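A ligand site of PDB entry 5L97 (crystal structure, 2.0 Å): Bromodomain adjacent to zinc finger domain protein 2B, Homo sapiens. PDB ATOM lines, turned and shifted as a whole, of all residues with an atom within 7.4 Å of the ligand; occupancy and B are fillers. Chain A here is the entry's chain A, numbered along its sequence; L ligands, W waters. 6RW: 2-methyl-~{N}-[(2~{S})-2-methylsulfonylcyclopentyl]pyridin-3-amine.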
ATOM      1  N   ALA A  31      -9.881  -9.633  16.404  1.00  0.00           N
ATOM      2  CA  ALA A  31      -9.233  -8.530  17.124  1.00  0.00           C
ATOM      3  C   ALA A  31      -8.603  -7.510  16.171  1.00  0.00           C
ATOM      4  O   ALA A  31      -8.298  -6.381  16.563  1.00  0.00           O
ATOM      5  CB  ALA A  31      -8.174  -9.061  18.083  1.00  0.00           C
ATOM      6  N   TRP A  32      -8.422  -7.921  14.912  1.00  0.00           N
ATOM      7  CA  TRP A  32      -7.676  -7.130  13.940  1.00  0.00           C
ATOM      8  C   TRP A  32      -8.040  -5.634  13.792  1.00  0.00           C
ATOM      9  O   TRP A  32      -7.149  -4.814  13.555  1.00  0.00           O
ATOM     10  CB  TRP A  32      -7.655  -7.818  12.564  1.00  0.00           C
ATOM     11  CG  TRP A  32      -9.016  -8.038  11.963  1.00  0.00           C
ATOM     12  CD1 TRP A  32      -9.797  -9.154  12.098  1.00  0.00           C
ATOM     13  CD2 TRP A  32      -9.742  -7.139  11.113  1.00  0.00           C
ATOM     14  NE1 TRP A  32     -10.967  -8.991  11.399  1.00  0.00           N
ATOM     15  CE2 TRP A  32     -10.957  -7.767  10.786  1.00  0.00           C
ATOM     16  CE3 TRP A  32      -9.487  -5.857  10.613  1.00  0.00           C
ATOM     17  CZ2 TRP A  32     -11.923  -7.160   9.973  1.00  0.00           C
ATOM     18  CZ3 TRP A  32     -10.437  -5.254   9.801  1.00  0.00           C
ATOM     19  CH2 TRP A  32     -11.641  -5.904   9.492  1.00  0.00           C
ATOM     20  N   PRO A  33      -9.336  -5.261  13.917  1.00  0.00           N
ATOM     21  CA  PRO A  33      -9.545  -3.830  13.728  1.00  0.00           C
ATOM     22  C   PRO A  33      -9.050  -3.007  14.919  1.00  0.00           C
ATOM     23  O   PRO A  33      -8.937  -1.786  14.797  1.00  0.00           O
ATOM     24  CB  PRO A  33     -11.074  -3.705  13.574  1.00  0.00           C
ATOM     25  CG  PRO A  33     -11.591  -5.127  13.374  1.00  0.00           C
ATOM     26  CD  PRO A  33     -10.607  -5.993  14.105  1.00  0.00           C
ATOM     27  N   PHE A  34      -8.761  -3.658  16.049  1.00  0.00           N
ATOM     28  CA  PHE A  34      -8.538  -2.962  17.318  1.00  0.00           C
ATOM     29  C   PHE A  34      -7.133  -3.088  17.880  1.00  0.00           C
ATOM     30  O   PHE A  34      -6.868  -2.658  19.024  1.00  0.00           O
ATOM     31  CB  PHE A  34      -9.534  -3.525  18.338  1.00  0.00           C
ATOM     32  CG  PHE A  34     -10.927  -3.669  17.787  1.00  0.00           C
ATOM     33  CD1 PHE A  34     -11.660  -2.548  17.438  1.00  0.00           C
ATOM     34  CD2 PHE A  34     -11.492  -4.926  17.603  1.00  0.00           C
ATOM     35  CE1 PHE A  34     -12.943  -2.672  16.912  1.00  0.00           C
ATOM     36  CE2 PHE A  34     -12.771  -5.057  17.082  1.00  0.00           C
ATOM     37  CZ  PHE A  34     -13.500  -3.923  16.731  1.00  0.00           C
ATOM     38  N   LEU A  35      -6.228  -3.690  17.109  1.00  0.00           N
ATOM     39  CA  LEU A  35      -4.896  -4.021  17.630  1.00  0.00           C
ATOM     40  C   LEU A  35      -4.030  -2.782  17.723  1.00  0.00           C
ATOM     41  O   LEU A  35      -3.169  -2.699  18.602  1.00  0.00           O
ATOM     42  CB  LEU A  35      -4.212  -5.085  16.768  1.00  0.00           C
ATOM     43  CG  LEU A  35      -4.851  -6.486  16.742  1.00  0.00           C
ATOM     44  CD1 LEU A  35      -4.095  -7.393  15.793  1.00  0.00           C
ATOM     45  CD2 LEU A  35      -4.872  -7.100  18.134  1.00  0.00           C
ATOM     46  N   LEU A  36      -4.254  -1.840  16.805  1.00  0.00           N
ATOM     47  CA  LEU A  36      -3.434  -0.634  16.690  1.00  0.00           C
ATOM     48  C   LEU A  36      -4.331   0.597  16.728  1.00  0.00           C
ATOM     49  O   LEU A  36      -5.547   0.461  16.601  1.00  0.00           O
ATOM     50  CB  LEU A  36      -2.606  -0.685  15.402  1.00  0.00           C
ATOM     51  CG  LEU A  36      -1.572  -1.805  15.281  1.00  0.00           C
ATOM     52  CD1 LEU A  36      -0.905  -1.737  13.915  1.00  0.00           C
ATOM     53  CD2 LEU A  36      -0.544  -1.718  16.394  1.00  0.00           C
ATOM     54  N   PRO A  37      -3.758   1.793  16.916  1.00  0.00           N
ATOM     55  CA  PRO A  37      -4.575   3.011  16.887  1.00  0.00           C
ATOM     56  C   PRO A  37      -5.123   3.228  15.480  1.00  0.00           C
ATOM     57  O   PRO A  37      -4.433   2.910  14.510  1.00  0.00           O
ATOM     58  CB  PRO A  37      -3.560   4.128  17.183  1.00  0.00           C
ATOM     59  CG  PRO A  37      -2.481   3.470  17.930  1.00  0.00           C
ATOM     60  CD  PRO A  37      -2.395   2.062  17.420  1.00  0.00           C
ATOM     61  N   VAL A  38      -6.336   3.749  15.358  1.00  0.00           N
ATOM     62  CA  VAL A  38      -6.849   4.154  14.049  1.00  0.00           C
ATOM     63  C   VAL A  38      -5.957   5.282  13.545  1.00  0.00           C
ATOM     64  O   VAL A  38      -5.609   6.183  14.299  1.00  0.00           O
ATOM     65  CB  VAL A  38      -8.309   4.616  14.131  1.00  0.00           C
ATOM     66  CG1 VAL A  38      -8.770   5.234  12.803  1.00  0.00           C
ATOM     67  CG2 VAL A  38      -9.208   3.445  14.515  1.00  0.00           C
ATOM     68  N   ASN A  39      -5.569   5.206  12.273  1.00  0.00           N
ATOM     69  CA  ASN A  39      -4.683   6.217  11.691  1.00  0.00           C
ATOM     70  C   ASN A  39      -5.460   7.493  11.431  1.00  0.00           C
ATOM     71  O   ASN A  39      -6.223   7.600  10.472  1.00  0.00           O
ATOM     72  CB  ASN A  39      -4.066   5.699  10.387  1.00  0.00           C
ATOM     73  CG  ASN A  39      -2.920   6.565   9.891  1.00  0.00           C
ATOM     74  OD1 ASN A  39      -2.955   7.794   9.996  1.00  0.00           O
ATOM     75  ND2 ASN A  39      -1.901   5.921   9.344  1.00  0.00           N
ATOM     76  N   LEU A  40      -5.254   8.486  12.305  1.00  0.00           N
ATOM     77  CA  LEU A  40      -6.027   9.723  12.237  1.00  0.00           C
ATOM     78  C   LEU A  40      -5.782  10.520  10.958  1.00  0.00           C
ATOM     79  O   LEU A  40      -6.565  11.402  10.612  1.00  0.00           O
ATOM     80  CB  LEU A  40      -5.768  10.595  13.465  1.00  0.00           C
ATOM     81  CG  LEU A  40      -6.204   9.947  14.776  1.00  0.00           C
ATOM     82  CD1 LEU A  40      -6.102  10.963  15.905  1.00  0.00           C
ATOM     83  CD2 LEU A  40      -7.613   9.375  14.662  1.00  0.00           C
ATOM     84  N   LEU A  42      -5.311   9.043   7.926  1.00  0.00           N
ATOM     85  CA  LEU A  42      -5.743   8.228   6.794  1.00  0.00           C
ATOM     86  C   LEU A  42      -7.246   7.973   6.799  1.00  0.00           C
ATOM     87  O   LEU A  42      -7.814   7.632   5.770  1.00  0.00           O
ATOM     88  CB  LEU A  42      -5.010   6.883   6.783  1.00  0.00           C
ATOM     89  CG  LEU A  42      -3.775   6.726   5.890  1.00  0.00           C
ATOM     90  CD1 LEU A  42      -2.835   7.912   6.008  1.00  0.00           C
ATOM     91  CD2 LEU A  42      -3.040   5.434   6.242  1.00  0.00           C
ATOM     92  N   VAL A  43      -7.888   8.119   7.953  1.00  0.00           N
ATOM     93  CA  VAL A  43      -9.316   7.838   8.052  1.00  0.00           C
ATOM     94  C   VAL A  43     -10.097   9.126   8.248  1.00  0.00           C
ATOM     95  O   VAL A  43     -10.123   9.667   9.349  1.00  0.00           O
ATOM     96  CB  VAL A  43      -9.640   6.860   9.198  1.00  0.00           C
ATOM     97  CG1 VAL A  43     -11.096   6.441   9.119  1.00  0.00           C
ATOM     98  CG2 VAL A  43      -8.719   5.647   9.133  1.00  0.00           C
ATOM     99  N   TYR A  46     -12.476  10.580  11.488  1.00  0.00           N
ATOM    100  CA  TYR A  46     -12.221   9.912  12.758  1.00  0.00           C
ATOM    101  C   TYR A  46     -11.771  10.860  13.877  1.00  0.00           C
ATOM    102  O   TYR A  46     -12.285  10.792  14.990  1.00  0.00           O
ATOM    103  CB  TYR A  46     -11.236   8.758  12.625  1.00  0.00           C
ATOM    104  CG  TYR A  46     -11.454   7.706  13.697  1.00  0.00           C
ATOM    105  CD1 TYR A  46     -10.715   7.713  14.871  1.00  0.00           C
ATOM    106  CD2 TYR A  46     -12.439   6.727  13.542  1.00  0.00           C
ATOM    107  CE1 TYR A  46     -10.910   6.744  15.861  1.00  0.00           C
ATOM    108  CE2 TYR A  46     -12.654   5.769  14.525  1.00  0.00           C
ATOM    109  CZ  TYR A  46     -11.887   5.787  15.676  1.00  0.00           C
ATOM    110  OH  TYR A  46     -12.110   4.824  16.656  1.00  0.00           O
ATOM    111  N   ILE A  50     -14.490  11.080  16.910  1.00  0.00           N
ATOM    112  CA  ILE A  50     -14.182  10.211  18.062  1.00  0.00           C
ATOM    113  C   ILE A  50     -13.277  10.954  19.031  1.00  0.00           C
ATOM    114  O   ILE A  50     -12.071  11.056  18.806  1.00  0.00           O
ATOM    115  CB  ILE A  50     -13.522   8.887  17.616  1.00  0.00           C
ATOM    116  CG1 ILE A  50     -14.434   8.118  16.652  1.00  0.00           C
ATOM    117  CG2 ILE A  50     -13.139   8.005  18.843  1.00  0.00           C
ATOM    118  CD1 ILE A  50     -15.792   7.816  17.223  1.00  0.00           C
ATOM    119  N   MET A  54      -9.149   4.748  21.316  1.00  0.00           N
ATOM    120  CA  MET A  54      -8.514   3.757  22.173  1.00  0.00           C
ATOM    121  C   MET A  54      -8.388   2.476  21.365  1.00  0.00           C
ATOM    122  O   MET A  54      -9.190   2.238  20.460  1.00  0.00           O
ATOM    123  CB  MET A  54      -9.330   3.550  23.454  1.00  0.00           C
ATOM    124  CG  MET A  54      -8.684   2.598  24.462  1.00  0.00           C
ATOM    125  SD  MET A  54      -7.024   3.163  24.918  1.00  0.00           S
ATOM    126  CE  MET A  54      -7.359   4.833  25.502  1.00  0.00           C
ATOM    127  N   ASP A  55      -7.362   1.684  21.675  1.00  0.00           N
ATOM    128  CA  ASP A  55      -7.132   0.406  20.999  1.00  0.00           C
ATOM    129  C   ASP A  55      -6.384  -0.518  21.942  1.00  0.00           C
ATOM    130  O   ASP A  55      -5.901  -0.064  22.979  1.00  0.00           O
ATOM    131  CB  ASP A  55      -6.311   0.636  19.727  1.00  0.00           C
ATOM    132  CG  ASP A  55      -4.911   1.118  20.029  1.00  0.00           C
ATOM    133  OD1 ASP A  55      -4.760   2.315  20.395  1.00  0.00           O
ATOM    134  OD2 ASP A  55      -3.966   0.321  19.909  1.00  0.00           O
ATOM    135  N   VAL A  81     -13.104   1.208  23.417  1.00  0.00           N
ATOM    136  CA  VAL A  81     -12.756   0.647  22.122  1.00  0.00           C
ATOM    137  C   VAL A  81     -14.014   0.257  21.324  1.00  0.00           C
ATOM    138  O   VAL A  81     -14.146   0.605  20.157  1.00  0.00           O
ATOM    139  CB  VAL A  81     -11.830  -0.585  22.240  1.00  0.00           C
ATOM    140  CG1 VAL A  81     -11.634  -1.243  20.880  1.00  0.00           C
ATOM    141  CG2 VAL A  81     -10.465  -0.203  22.873  1.00  0.00           C
ATOM    142  N   ASN A  84     -16.472   3.339  20.587  1.00  0.00           N
ATOM    143  CA  ASN A  84     -15.960   4.069  19.420  1.00  0.00           C
ATOM    144  C   ASN A  84     -16.293   3.332  18.135  1.00  0.00           C
ATOM    145  O   ASN A  84     -16.711   3.928  17.153  1.00  0.00           O
ATOM    146  CB  ASN A  84     -14.442   4.245  19.498  1.00  0.00           C
ATOM    147  CG  ASN A  84     -14.006   5.203  20.602  1.00  0.00           C
ATOM    148  OD1 ASN A  84     -14.808   5.982  21.117  1.00  0.00           O
ATOM    149  ND2 ASN A  84     -12.717   5.156  20.938  1.00  0.00           N
ATOM    150  N   CYS A  85     -16.100   2.014  18.147  1.00  0.00           N
ATOM    151  CA  CYS A  85     -16.361   1.197  16.975  1.00  0.00           C
ATOM    152  C   CYS A  85     -17.817   1.332  16.543  1.00  0.00           C
ATOM    153  O   CYS A  85     -18.109   1.474  15.350  1.00  0.00           O
ATOM    154  CB  CYS A  85     -15.995  -0.279  17.236  1.00  0.00           C
ATOM    155  SG  CYS A  85     -16.288  -1.399  15.831  1.00  0.00           S
ATOM    156  N   PHE A  88     -18.611   4.783  14.849  1.00  0.00           N
ATOM    157  CA  PHE A  88     -18.042   5.043  13.530  1.00  0.00           C
ATOM    158  C   PHE A  88     -18.439   4.017  12.469  1.00  0.00           C
ATOM    159  O   PHE A  88     -18.451   4.334  11.275  1.00  0.00           O
ATOM    160  CB  PHE A  88     -16.512   5.152  13.617  1.00  0.00           C
ATOM    161  CG  PHE A  88     -15.903   6.003  12.529  1.00  0.00           C
ATOM    162  CD1 PHE A  88     -16.003   7.384  12.591  1.00  0.00           C
ATOM    163  CD2 PHE A  88     -15.266   5.425  11.450  1.00  0.00           C
ATOM    164  CE1 PHE A  88     -15.451   8.178  11.587  1.00  0.00           C
ATOM    165  CE2 PHE A  88     -14.707   6.204  10.458  1.00  0.00           C
ATOM    166  CZ  PHE A  88     -14.811   7.592  10.514  1.00  0.00           C
ATOM    167  N   ASN A  89     -18.778   2.805  12.903  1.00  0.00           N
ATOM    168  CA  ASN A  89     -19.016   1.698  11.971  1.00  0.00           C
ATOM    169  C   ASN A  89     -20.458   1.172  11.972  1.00  0.00           C
ATOM    170  O   ASN A  89     -21.071   1.054  13.029  1.00  0.00           O
ATOM    171  CB  ASN A  89     -18.064   0.532  12.281  1.00  0.00           C
ATOM    172  CG  ASN A  89     -16.582   0.935  12.201  1.00  0.00           C
ATOM    173  OD1 ASN A  89     -15.987   0.906  11.122  1.00  0.00           O
ATOM    174  ND2 ASN A  89     -15.989   1.268  13.344  1.00  0.00           N
ATOM    175  N   ILE A  95     -16.052  -4.658  10.327  1.00  0.00           N
ATOM    176  CA  ILE A  95     -15.524  -4.049  11.535  1.00  0.00           C
ATOM    177  C   ILE A  95     -16.618  -3.922  12.600  1.00  0.00           C
ATOM    178  O   ILE A  95     -16.390  -4.222  13.768  1.00  0.00           O
ATOM    179  CB  ILE A  95     -14.923  -2.657  11.257  1.00  0.00           C
ATOM    180  CG1 ILE A  95     -13.687  -2.784  10.366  1.00  0.00           C
ATOM    181  CG2 ILE A  95     -14.556  -1.950  12.554  1.00  0.00           C
ATOM    182  CD1 ILE A  95     -13.157  -1.457   9.874  1.00  0.00           C
HETATM  183  C10 6RW L   1      -9.625  -1.228  10.011  1.00  0.00           C
HETATM  184  C11 6RW L   1      -8.705  -2.163   9.676  1.00  0.00           C
HETATM  185  C12 6RW L   1      -7.527  -1.978  10.733  1.00  0.00           C
HETATM  186  C13 6RW L   1      -7.523  -0.357  10.883  1.00  0.00           C
HETATM  187  C01 6RW L   1     -11.568   0.032  14.339  1.00  0.00           C
HETATM  188  C02 6RW L   1     -11.628   1.002  13.178  1.00  0.00           C
HETATM  189  C03 6RW L   1     -10.652   1.016  12.177  1.00  0.00           C
HETATM  190  C04 6RW L   1     -10.772   1.929  11.139  1.00  0.00           C
HETATM  191  C05 6RW L   1     -11.855   2.799  11.124  1.00  0.00           C
HETATM  192  C06 6RW L   1     -12.787   2.754  12.145  1.00  0.00           C
HETATM  193  N07 6RW L   1     -12.660   1.854  13.144  1.00  0.00           N
HETATM  194  N08 6RW L   1      -9.531   0.121  12.153  1.00  0.00           N
HETATM  195  C09 6RW L   1      -8.868  -0.014  10.930  1.00  0.00           C
HETATM  196  S14 6RW L   1      -6.312   0.254  12.153  1.00  0.00           S
HETATM  197  O15 6RW L   1      -5.581   1.395  11.679  1.00  0.00           O
HETATM  198  O16 6RW L   1      -5.244  -0.700  12.296  1.00  0.00           O
HETATM  199  C17 6RW L   1      -7.029   0.612  13.734  1.00  0.00           C
HETATM  200  O   HOH W   1     -13.510   2.685  15.823  1.00  0.00           O
HETATM  201  O   HOH W   2      -5.530  -2.695  14.207  1.00  0.00           O
HETATM  202  O   HOH W   3      -6.408   3.409  10.425  1.00  0.00           O
HETATM  203  O   HOH W   4      -8.523   0.541  16.582  1.00  0.00           O
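A nitrogen (N08) of the ligand sits close to the backbone carbonyl oxygen (O) of Pro 33 (3.3 Å).
The side-chain amide nitrogen (ND2) of Asn 89 is in hydrogen-bond range of a nitrogen (N07) of the ligand (3.4 Å).
O of Ile 95 is in hydrogen-bond range of SG of Cys 85 (3.5 Å).
The backbone carbonyl oxygen (O) of Cys 85 is in hydrogen-bond range of the side-chain amide nitrogen (ND2) of Asn 89.
The backbone NH of Leu 42 is in hydrogen-bond range of the side-chain amide oxygen of Asn 39 (3.4 Å).
An oxygen (O15) of the ligand lies close to the backbone carbonyl oxygen (O) of Pro 37 (3.4 Å).
Trp 32 touches the ligand (CZ3 to C11, 3.5 Å).
CE1 of Phe 34 touches C01 of the ligand, at 3.98 Å.
O of Leu 36 touches C17 of the ligand, at 3.2 Å.
Val 38 touches the ligand.
Asn 39 touches the ligand (N to O15, 3.9 Å).
Tyr 46 touches the ligand.
Phe 88 touches the ligand (CD2 to C06, 3.7 Å).
Ile 95 touches the ligand (CD1 to C10, 3.5 Å).
Hydrophobic or aromatic side chains within 4 Å of the ligand: Trp 32, Pro 33, Phe 34, Val 38, Tyr 46, Phe 88 and Ile 95.
Within 4 Å of the ligand: Trp 32, Pro 33, Phe 34, Leu 36, Pro 37, Val 38, Asn 39, Tyr 46, Phe 88, Asn 89 and Ile 95.
The nearest printed residue that does not touch the ligand is Val 43 (4.2 Å).
Water W3 lies within hydrogen-bond range of an oxygen (O15) of the ligand and the backbone NH (N) of Asn 39.
Water W2 lies within hydrogen-bond range of the backbone carbonyl oxygen (O) of Trp 32 (2.7 Å), an oxygen (O16) of the ligand (2.8 Å), the backbone NH (N) of Leu 36 (3.0 Å) and the backbone NH (N) of Leu 35 (3.1 Å).
Water W1 bridges OH of Tyr 46 and N07 of the ligand.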
